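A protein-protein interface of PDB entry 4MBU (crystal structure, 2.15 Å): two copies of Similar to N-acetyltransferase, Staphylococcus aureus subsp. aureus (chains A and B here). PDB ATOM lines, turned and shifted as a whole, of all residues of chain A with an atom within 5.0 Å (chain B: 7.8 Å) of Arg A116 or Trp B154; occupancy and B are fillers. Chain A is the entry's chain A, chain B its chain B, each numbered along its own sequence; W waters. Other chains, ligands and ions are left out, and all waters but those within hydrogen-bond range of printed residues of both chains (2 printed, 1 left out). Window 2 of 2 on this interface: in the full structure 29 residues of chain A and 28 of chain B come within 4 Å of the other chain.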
ATOM      1  N   TYR A  81      26.601  -8.883  21.999  1.00  0.00           N
ATOM      2  CA  TYR A  81      25.496  -9.189  21.089  1.00  0.00           C
ATOM      3  C   TYR A  81      24.871  -7.942  20.450  1.00  0.00           C
ATOM      4  O   TYR A  81      23.869  -8.031  19.730  1.00  0.00           O
ATOM      5  CB  TYR A  81      24.451 -10.064  21.774  1.00  0.00           C
ATOM      6  CG  TYR A  81      25.030 -11.347  22.291  1.00  0.00           C
ATOM      7  CD1 TYR A  81      25.485 -12.325  21.419  1.00  0.00           C
ATOM      8  CD2 TYR A  81      25.134 -11.584  23.655  1.00  0.00           C
ATOM      9  CE1 TYR A  81      26.025 -13.507  21.895  1.00  0.00           C
ATOM     10  CE2 TYR A  81      25.667 -12.760  24.139  1.00  0.00           C
ATOM     11  CZ  TYR A  81      26.112 -13.719  23.255  1.00  0.00           C
ATOM     12  OH  TYR A  81      26.643 -14.896  23.734  1.00  0.00           O
ATOM     13  N   GLY A 114      24.113 -14.013  14.469  1.00  0.00           N
ATOM     14  CA  GLY A 114      23.605 -14.249  15.811  1.00  0.00           C
ATOM     15  C   GLY A 114      23.584 -13.066  16.770  1.00  0.00           C
ATOM     16  O   GLY A 114      23.516 -13.256  17.987  1.00  0.00           O
ATOM     17  N   TYR A 115      23.646 -11.843  16.250  1.00  0.00           N
ATOM     18  CA  TYR A 115      23.549 -10.685  17.127  1.00  0.00           C
ATOM     19  C   TYR A 115      22.119 -10.556  17.646  1.00  0.00           C
ATOM     20  O   TYR A 115      21.193 -11.154  17.091  1.00  0.00           O
ATOM     21  CB  TYR A 115      24.029  -9.414  16.412  1.00  0.00           C
ATOM     22  CG  TYR A 115      25.517  -9.454  16.109  1.00  0.00           C
ATOM     23  CD1 TYR A 115      26.446  -9.248  17.116  1.00  0.00           C
ATOM     24  CD2 TYR A 115      25.988  -9.718  14.821  1.00  0.00           C
ATOM     25  CE1 TYR A 115      27.803  -9.286  16.858  1.00  0.00           C
ATOM     26  CE2 TYR A 115      27.357  -9.757  14.549  1.00  0.00           C
ATOM     27  CZ  TYR A 115      28.251  -9.542  15.578  1.00  0.00           C
ATOM     28  OH  TYR A 115      29.605  -9.571  15.346  1.00  0.00           O
ATOM     29  N   ARG A 116      21.940  -9.796  18.721  1.00  0.00           N
ATOM     30  CA  ARG A 116      20.621  -9.632  19.327  1.00  0.00           C
ATOM     31  C   ARG A 116      20.033  -8.273  18.995  1.00  0.00           C
ATOM     32  O   ARG A 116      18.828  -8.146  18.751  1.00  0.00           O
ATOM     33  CB  ARG A 116      20.710  -9.774  20.852  1.00  0.00           C
ATOM     34  CG  ARG A 116      19.375  -9.468  21.582  1.00  0.00           C
ATOM     35  CD  ARG A 116      18.291 -10.461  21.166  1.00  0.00           C
ATOM     36  NE  ARG A 116      16.939 -10.080  21.579  1.00  0.00           N
ATOM     37  CZ  ARG A 116      16.386 -10.406  22.748  1.00  0.00           C
ATOM     38  NH1 ARG A 116      17.077 -11.100  23.648  1.00  0.00           N
ATOM     39  NH2 ARG A 116      15.142 -10.024  23.026  1.00  0.00           N
ATOM     40  N   THR A 117      20.892  -7.255  18.998  1.00  0.00           N
ATOM     41  CA  THR A 117      20.433  -5.870  18.964  1.00  0.00           C
ATOM     42  C   THR A 117      21.237  -5.039  17.973  1.00  0.00           C
ATOM     43  O   THR A 117      22.478  -4.979  18.050  1.00  0.00           O
ATOM     44  CB  THR A 117      20.514  -5.238  20.371  1.00  0.00           C
ATOM     45  OG1 THR A 117      19.689  -5.997  21.270  1.00  0.00           O
ATOM     46  CG2 THR A 117      20.048  -3.783  20.349  1.00  0.00           C
ATOM     47  N   LEU A 118      20.526  -4.414  17.032  1.00  0.00           N
ATOM     48  CA  LEU A 118      21.158  -3.537  16.041  1.00  0.00           C
ATOM     49  C   LEU A 118      20.801  -2.080  16.342  1.00  0.00           C
ATOM     50  O   LEU A 118      19.619  -1.726  16.448  1.00  0.00           O
ATOM     51  CB  LEU A 118      20.728  -3.935  14.620  1.00  0.00           C
ATOM     52  CG  LEU A 118      21.288  -3.171  13.408  1.00  0.00           C
ATOM     53  CD1 LEU A 118      22.799  -3.258  13.402  1.00  0.00           C
ATOM     54  CD2 LEU A 118      20.732  -3.745  12.113  1.00  0.00           C
ATOM     55  N   LEU A 162      16.760  -2.094  16.676  1.00  0.00           N
ATOM     56  CA  LEU A 162      16.017  -3.259  16.218  1.00  0.00           C
ATOM     57  C   LEU A 162      16.407  -4.479  17.032  1.00  0.00           C
ATOM     58  O   LEU A 162      17.607  -4.811  17.147  1.00  0.00           O
ATOM     59  CB  LEU A 162      16.323  -3.520  14.748  1.00  0.00           C
ATOM     60  CG  LEU A 162      15.715  -4.758  14.094  1.00  0.00           C
ATOM     61  CD1 LEU A 162      14.185  -4.648  14.031  1.00  0.00           C
ATOM     62  CD2 LEU A 162      16.300  -4.936  12.702  1.00  0.00           C
ATOM     63  N   ASP A 163      15.392  -5.133  17.603  1.00  0.00           N
ATOM     64  CA  ASP A 163      15.553  -6.452  18.208  1.00  0.00           C
ATOM     65  C   ASP A 163      15.587  -7.488  17.093  1.00  0.00           C
ATOM     66  O   ASP A 163      14.572  -7.735  16.427  1.00  0.00           O
ATOM     67  CB  ASP A 163      14.391  -6.782  19.150  1.00  0.00           C
ATOM     68  CG  ASP A 163      14.644  -8.057  19.965  1.00  0.00           C
ATOM     69  OD1 ASP A 163      15.601  -8.809  19.647  1.00  0.00           O
ATOM     70  OD2 ASP A 163      13.897  -8.312  20.932  1.00  0.00           O
ATOM     71  N   LEU A 164      16.755  -8.097  16.901  1.00  0.00           N
ATOM     72  CA  LEU A 164      16.951  -9.076  15.837  1.00  0.00           C
ATOM     73  C   LEU A 164      16.349 -10.470  16.125  1.00  0.00           C
ATOM     74  O   LEU A 164      16.338 -11.333  15.238  1.00  0.00           O
ATOM     75  CB  LEU A 164      18.443  -9.207  15.535  1.00  0.00           C
ATOM     76  CG  LEU A 164      19.156  -7.918  15.149  1.00  0.00           C
ATOM     77  CD1 LEU A 164      20.641  -8.164  15.109  1.00  0.00           C
ATOM     78  CD2 LEU A 164      18.665  -7.459  13.804  1.00  0.00           C
ATOM     79  N   LYS A 165      15.859 -10.684  17.348  1.00  0.00           N
ATOM     80  CA  LYS A 165      15.302 -11.987  17.748  1.00  0.00           C
ATOM     81  C   LYS A 165      13.883 -12.182  17.226  1.00  0.00           C
ATOM     82  O   LYS A 165      13.055 -11.275  17.314  1.00  0.00           O
ATOM     83  CB  LYS A 165      15.329 -12.139  19.278  1.00  0.00           C
ATOM     84  CG  LYS A 165      14.757 -13.457  19.807  1.00  0.00           C
ATOM     85  CD  LYS A 165      15.064 -13.669  21.301  1.00  0.00           C
ATOM     86  CE  LYS A 165      14.655 -15.071  21.771  1.00  0.00           C
ATOM     87  NZ  LYS A 165      15.391 -15.515  22.994  1.00  0.00           N
ATOM     88  N   THR B  28      26.033  -5.424  37.703  1.00  0.00           N
ATOM     89  CA  THR B  28      25.888  -5.019  36.309  1.00  0.00           C
ATOM     90  C   THR B  28      26.413  -3.604  36.084  1.00  0.00           C
ATOM     91  O   THR B  28      26.192  -3.011  35.029  1.00  0.00           O
ATOM     92  CB  THR B  28      24.410  -5.060  35.890  1.00  0.00           C
ATOM     93  OG1 THR B  28      23.660  -4.175  36.723  1.00  0.00           O
ATOM     94  CG2 THR B  28      23.857  -6.461  36.064  1.00  0.00           C
ATOM     95  N   TYR B  31      29.979  -3.560  32.389  1.00  0.00           N
ATOM     96  CA  TYR B  31      29.654  -4.558  31.359  1.00  0.00           C
ATOM     97  C   TYR B  31      30.881  -5.391  30.926  1.00  0.00           C
ATOM     98  O   TYR B  31      31.199  -5.498  29.738  1.00  0.00           O
ATOM     99  CB  TYR B  31      28.984  -3.903  30.141  1.00  0.00           C
ATOM    100  CG  TYR B  31      27.519  -3.527  30.326  1.00  0.00           C
ATOM    101  CD1 TYR B  31      26.987  -3.310  31.584  1.00  0.00           C
ATOM    102  CD2 TYR B  31      26.668  -3.422  29.233  1.00  0.00           C
ATOM    103  CE1 TYR B  31      25.650  -2.969  31.748  1.00  0.00           C
ATOM    104  CE2 TYR B  31      25.337  -3.078  29.385  1.00  0.00           C
ATOM    105  CZ  TYR B  31      24.833  -2.849  30.643  1.00  0.00           C
ATOM    106  OH  TYR B  31      23.503  -2.511  30.810  1.00  0.00           O
ATOM    107  N   ASP B 123      22.830   1.212  34.316  1.00  0.00           N
ATOM    108  CA  ASP B 123      22.041   0.002  34.113  1.00  0.00           C
ATOM    109  C   ASP B 123      20.637   0.243  34.655  1.00  0.00           C
ATOM    110  O   ASP B 123      20.470   0.811  35.740  1.00  0.00           O
ATOM    111  CB  ASP B 123      22.680  -1.220  34.776  1.00  0.00           C
ATOM    112  CG  ASP B 123      21.954  -2.509  34.424  1.00  0.00           C
ATOM    113  OD1 ASP B 123      22.174  -3.021  33.300  1.00  0.00           O
ATOM    114  OD2 ASP B 123      21.152  -2.994  35.260  1.00  0.00           O
ATOM    115  N   THR B 145      17.351  -1.227  25.093  1.00  0.00           N
ATOM    116  CA  THR B 145      16.981  -2.513  25.676  1.00  0.00           C
ATOM    117  C   THR B 145      17.815  -3.640  25.083  1.00  0.00           C
ATOM    118  O   THR B 145      18.133  -3.616  23.888  1.00  0.00           O
ATOM    119  CB  THR B 145      15.499  -2.817  25.419  1.00  0.00           C
ATOM    120  OG1 THR B 145      15.218  -2.564  24.042  1.00  0.00           O
ATOM    121  CG2 THR B 145      14.620  -1.902  26.260  1.00  0.00           C
ATOM    122  N   ASN B 146      18.148  -4.622  25.921  1.00  0.00           N
ATOM    123  CA  ASN B 146      18.879  -5.809  25.499  1.00  0.00           C
ATOM    124  C   ASN B 146      20.230  -5.473  24.890  1.00  0.00           C
ATOM    125  O   ASN B 146      20.676  -6.155  23.961  1.00  0.00           O
ATOM    126  CB  ASN B 146      18.048  -6.619  24.484  1.00  0.00           C
ATOM    127  CG  ASN B 146      16.679  -7.018  25.024  1.00  0.00           C
ATOM    128  OD1 ASN B 146      16.547  -7.431  26.175  1.00  0.00           O
ATOM    129  ND2 ASN B 146      15.653  -6.901  24.183  1.00  0.00           N
ATOM    130  N   VAL B 147      20.878  -4.414  25.377  1.00  0.00           N
ATOM    131  CA  VAL B 147      22.168  -4.038  24.804  1.00  0.00           C
ATOM    132  C   VAL B 147      23.290  -4.791  25.468  1.00  0.00           C
ATOM    133  O   VAL B 147      24.378  -4.902  24.897  1.00  0.00           O
ATOM    134  CB  VAL B 147      22.501  -2.528  24.930  1.00  0.00           C
ATOM    135  CG1 VAL B 147      21.875  -1.742  23.806  1.00  0.00           C
ATOM    136  CG2 VAL B 147      22.118  -2.005  26.305  1.00  0.00           C
ATOM    137  N   GLY B 148      23.041  -5.279  26.687  1.00  0.00           N
ATOM    138  CA  GLY B 148      24.074  -6.019  27.396  1.00  0.00           C
ATOM    139  C   GLY B 148      23.629  -7.435  27.737  1.00  0.00           C
ATOM    140  O   GLY B 148      22.441  -7.747  27.671  1.00  0.00           O
ATOM    141  N   TYR B 149      24.578  -8.295  28.093  1.00  0.00           N
ATOM    142  CA  TYR B 149      24.257  -9.656  28.527  1.00  0.00           C
ATOM    143  C   TYR B 149      25.227 -10.093  29.613  1.00  0.00           C
ATOM    144  O   TYR B 149      26.433 -10.212  29.381  1.00  0.00           O
ATOM    145  CB  TYR B 149      24.314 -10.634  27.349  1.00  0.00           C
ATOM    146  CG  TYR B 149      23.830 -12.046  27.663  1.00  0.00           C
ATOM    147  CD1 TYR B 149      22.472 -12.344  27.706  1.00  0.00           C
ATOM    148  CD2 TYR B 149      24.730 -13.080  27.881  1.00  0.00           C
ATOM    149  CE1 TYR B 149      22.023 -13.627  27.973  1.00  0.00           C
ATOM    150  CE2 TYR B 149      24.292 -14.370  28.144  1.00  0.00           C
ATOM    151  CZ  TYR B 149      22.939 -14.636  28.187  1.00  0.00           C
ATOM    152  OH  TYR B 149      22.489 -15.911  28.453  1.00  0.00           O
ATOM    153  N   LYS B 150      24.696 -10.343  30.798  1.00  0.00           N
ATOM    154  CA  LYS B 150      25.540 -10.698  31.933  1.00  0.00           C
ATOM    155  C   LYS B 150      24.711 -11.482  32.956  1.00  0.00           C
ATOM    156  O   LYS B 150      23.501 -11.258  33.082  1.00  0.00           O
ATOM    157  CB  LYS B 150      26.142  -9.430  32.548  1.00  0.00           C
ATOM    158  CG  LYS B 150      27.203  -9.691  33.617  1.00  0.00           C
ATOM    159  CD  LYS B 150      27.920  -8.394  34.048  1.00  0.00           C
ATOM    160  CE  LYS B 150      29.131  -8.731  34.932  1.00  0.00           C
ATOM    161  NZ  LYS B 150      29.779  -7.521  35.513  1.00  0.00           N
ATOM    162  N   PHE B 151      25.356 -12.425  33.644  1.00  0.00           N
ATOM    163  CA  PHE B 151      24.678 -13.253  34.652  1.00  0.00           C
ATOM    164  C   PHE B 151      23.493 -13.993  34.033  1.00  0.00           C
ATOM    165  O   PHE B 151      22.464 -14.182  34.690  1.00  0.00           O
ATOM    166  CB  PHE B 151      24.198 -12.392  35.828  1.00  0.00           C
ATOM    167  CG  PHE B 151      25.307 -11.656  36.544  1.00  0.00           C
ATOM    168  CD1 PHE B 151      26.545 -12.253  36.737  1.00  0.00           C
ATOM    169  CD2 PHE B 151      25.110 -10.367  37.018  1.00  0.00           C
ATOM    170  CE1 PHE B 151      27.563 -11.584  37.404  1.00  0.00           C
ATOM    171  CE2 PHE B 151      26.128  -9.691  37.680  1.00  0.00           C
ATOM    172  CZ  PHE B 151      27.349 -10.302  37.870  1.00  0.00           C
ATOM    173  N   ASP B 152      23.633 -14.375  32.761  1.00  0.00           N
ATOM    174  CA  ASP B 152      22.597 -15.119  32.028  1.00  0.00           C
ATOM    175  C   ASP B 152      21.310 -14.368  31.738  1.00  0.00           C
ATOM    176  O   ASP B 152      20.290 -14.993  31.437  1.00  0.00           O
ATOM    177  CB  ASP B 152      22.225 -16.403  32.760  1.00  0.00           C
ATOM    178  CG  ASP B 152      23.419 -17.256  33.056  1.00  0.00           C
ATOM    179  OD1 ASP B 152      24.286 -17.355  32.174  1.00  0.00           O
ATOM    180  OD2 ASP B 152      23.485 -17.789  34.174  1.00  0.00           O
ATOM    181  N   TYR B 153      21.333 -13.043  31.813  1.00  0.00           N
ATOM    182  CA  TYR B 153      20.160 -12.297  31.365  1.00  0.00           C
ATOM    183  C   TYR B 153      20.468 -11.017  30.587  1.00  0.00           C
ATOM    184  O   TYR B 153      21.589 -10.499  30.614  1.00  0.00           O
ATOM    185  CB  TYR B 153      19.166 -12.054  32.510  1.00  0.00           C
ATOM    186  CG  TYR B 153      19.789 -11.516  33.772  1.00  0.00           C
ATOM    187  CD1 TYR B 153      19.899 -12.306  34.907  1.00  0.00           C
ATOM    188  CD2 TYR B 153      20.264 -10.208  33.828  1.00  0.00           C
ATOM    189  CE1 TYR B 153      20.472 -11.808  36.065  1.00  0.00           C
ATOM    190  CE2 TYR B 153      20.834  -9.701  34.977  1.00  0.00           C
ATOM    191  CZ  TYR B 153      20.938 -10.503  36.091  1.00  0.00           C
ATOM    192  OH  TYR B 153      21.512  -9.992  37.235  1.00  0.00           O
ATOM    193  N   TRP B 154      19.456 -10.528  29.883  1.00  0.00           N
ATOM    194  CA  TRP B 154      19.603  -9.376  29.016  1.00  0.00           C
ATOM    195  C   TRP B 154      19.534  -8.088  29.834  1.00  0.00           C
ATOM    196  O   TRP B 154      18.740  -7.978  30.766  1.00  0.00           O
ATOM    197  CB  TRP B 154      18.534  -9.419  27.930  1.00  0.00           C
ATOM    198  CG  TRP B 154      18.766 -10.572  26.999  1.00  0.00           C
ATOM    199  CD1 TRP B 154      18.092 -11.764  26.970  1.00  0.00           C
ATOM    200  CD2 TRP B 154      19.778 -10.655  25.984  1.00  0.00           C
ATOM    201  NE1 TRP B 154      18.620 -12.577  25.988  1.00  0.00           N
ATOM    202  CE2 TRP B 154      19.654 -11.921  25.369  1.00  0.00           C
ATOM    203  CE3 TRP B 154      20.772  -9.776  25.533  1.00  0.00           C
ATOM    204  CZ2 TRP B 154      20.484 -12.330  24.323  1.00  0.00           C
ATOM    205  CZ3 TRP B 154      21.597 -10.181  24.501  1.00  0.00           C
ATOM    206  CH2 TRP B 154      21.451 -11.450  23.907  1.00  0.00           C
ATOM    207  N   LEU B 155      20.385  -7.128  29.480  1.00  0.00           N
ATOM    208  CA  LEU B 155      20.547  -5.889  30.229  1.00  0.00           C
ATOM    209  C   LEU B 155      20.124  -4.685  29.396  1.00  0.00           C
ATOM    210  O   LEU B 155      20.472  -4.588  28.199  1.00  0.00           O
ATOM    211  CB  LEU B 155      22.011  -5.695  30.633  1.00  0.00           C
ATOM    212  CG  LEU B 155      22.768  -6.811  31.349  1.00  0.00           C
ATOM    213  CD1 LEU B 155      24.181  -6.338  31.648  1.00  0.00           C
ATOM    214  CD2 LEU B 155      22.050  -7.209  32.640  1.00  0.00           C
ATOM    215  N   ASP B 156      19.411  -3.769  30.059  1.00  0.00           N
ATOM    216  CA  ASP B 156      18.975  -2.505  29.477  1.00  0.00           C
ATOM    217  C   ASP B 156      19.833  -1.357  30.020  1.00  0.00           C
ATOM    218  O   ASP B 156      20.070  -1.261  31.222  1.00  0.00           O
ATOM    219  CB  ASP B 156      17.501  -2.242  29.810  1.00  0.00           C
ATOM    220  CG  ASP B 156      16.581  -3.378  29.377  1.00  0.00           C
ATOM    221  OD1 ASP B 156      16.957  -4.164  28.487  1.00  0.00           O
ATOM    222  OD2 ASP B 156      15.470  -3.479  29.933  1.00  0.00           O
ATOM    223  N   LEU B 157      20.297  -0.488  29.130  1.00  0.00           N
ATOM    224  CA  LEU B 157      21.129   0.634  29.531  1.00  0.00           C
ATOM    225  C   LEU B 157      20.345   1.924  29.389  1.00  0.00           C
ATOM    226  O   LEU B 157      19.904   2.272  28.304  1.00  0.00           O
ATOM    227  CB  LEU B 157      22.383   0.706  28.662  1.00  0.00           C
ATOM    228  CG  LEU B 157      23.385   1.795  29.051  1.00  0.00           C
ATOM    229  CD1 LEU B 157      24.188   1.367  30.278  1.00  0.00           C
ATOM    230  CD2 LEU B 157      24.306   2.117  27.879  1.00  0.00           C
HETATM  231  O   HOH W   1      14.968  -9.938  26.468  1.00  0.00           O
HETATM  232  O   HOH W   2      25.450  -8.093  24.250  1.00  0.00           O
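No position is printed for both chains.
Of the 16 printed residues of chain B, 4 touch a printed residue of chain A.
Of the printed residues of chain B, Tyr A81 touches Tyr B149 (3.9 Å) and Trp B154 (3.7 Å). Arg A116 touches just these residues of chain B: Asn B146 (3.4 Å) and Trp B154 (3.2 Å). Of the printed residues of chain B, Thr A117 touches Thr B145 (3.9 Å) and Asn B146 (2.9 Å). Printed residues of chain A within 4 Å of Asn B146: Arg A116 (3.4 Å), Thr A117 (2.9 Å) and Asp A163 (3.96 Å). Val B147 touches none of the printed residues of chain A. Gly B148 touches none of the printed residues of chain A. Of the printed residues of chain A, Trp B154 touches Tyr A81 and Arg A116. The nearest residue of chain B that does not touch Arg A116 is Thr B145 (6.4 Å). The nearest printed residue of chain B that does not touch Thr A117 is Val B147 (4.4 Å).
NH2 of Arg A116 lies close to ND2 of Asn B146 (3.4 Å). O of Asn B146 sits at hydrogen-bond distance from OG1 of Thr A117 (2.9 Å). NE1 of Trp B154 sits close to NH1 of Arg A116 (3.2 Å).
O of Arg A116 is in hydrogen-bond range of N of Leu A164 (2.8 Å). N of Asn B146 lies within hydrogen-bond range of OD1 of Asp B156 (2.9 Å). The backbone NH (N) of Lys A165 is in hydrogen-bond range of the side-chain carboxylate (OD1) of Asp A163 (3.0 Å). The backbone carbonyl oxygen of Leu B155 is in hydrogen-bond range of the backbone NH of Asn B146, at 3.3 Å. NE of Arg A116 lies within salt-bridge range of OD1 of Asp A163 (2.7 Å). The backbone carbonyl oxygen of Tyr A81 lies within hydrogen-bond range of the backbone NH of Thr A117, at 3.2 Å.
Tyr A81 touches Tyr B149 (CE2 to CD2, 3.9 Å). CD2 of Tyr A81 touches CH2 of Trp B154, at 3.7 Å. Thr A117 touches Thr B145 (OG1 to O, 3.9 Å). OD2 of Asp A163 touches ND2 of Asn B146, at 3.96 Å.
Water W2 bridges the backbone NH (N) of Tyr A81 and the backbone carbonyl oxygen (O) of Val B147. Water W1 bridges the side-chain amide oxygen of Asn B146 (3.0 Å) and the guanidinium group of Arg A116 (3.4 Å).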
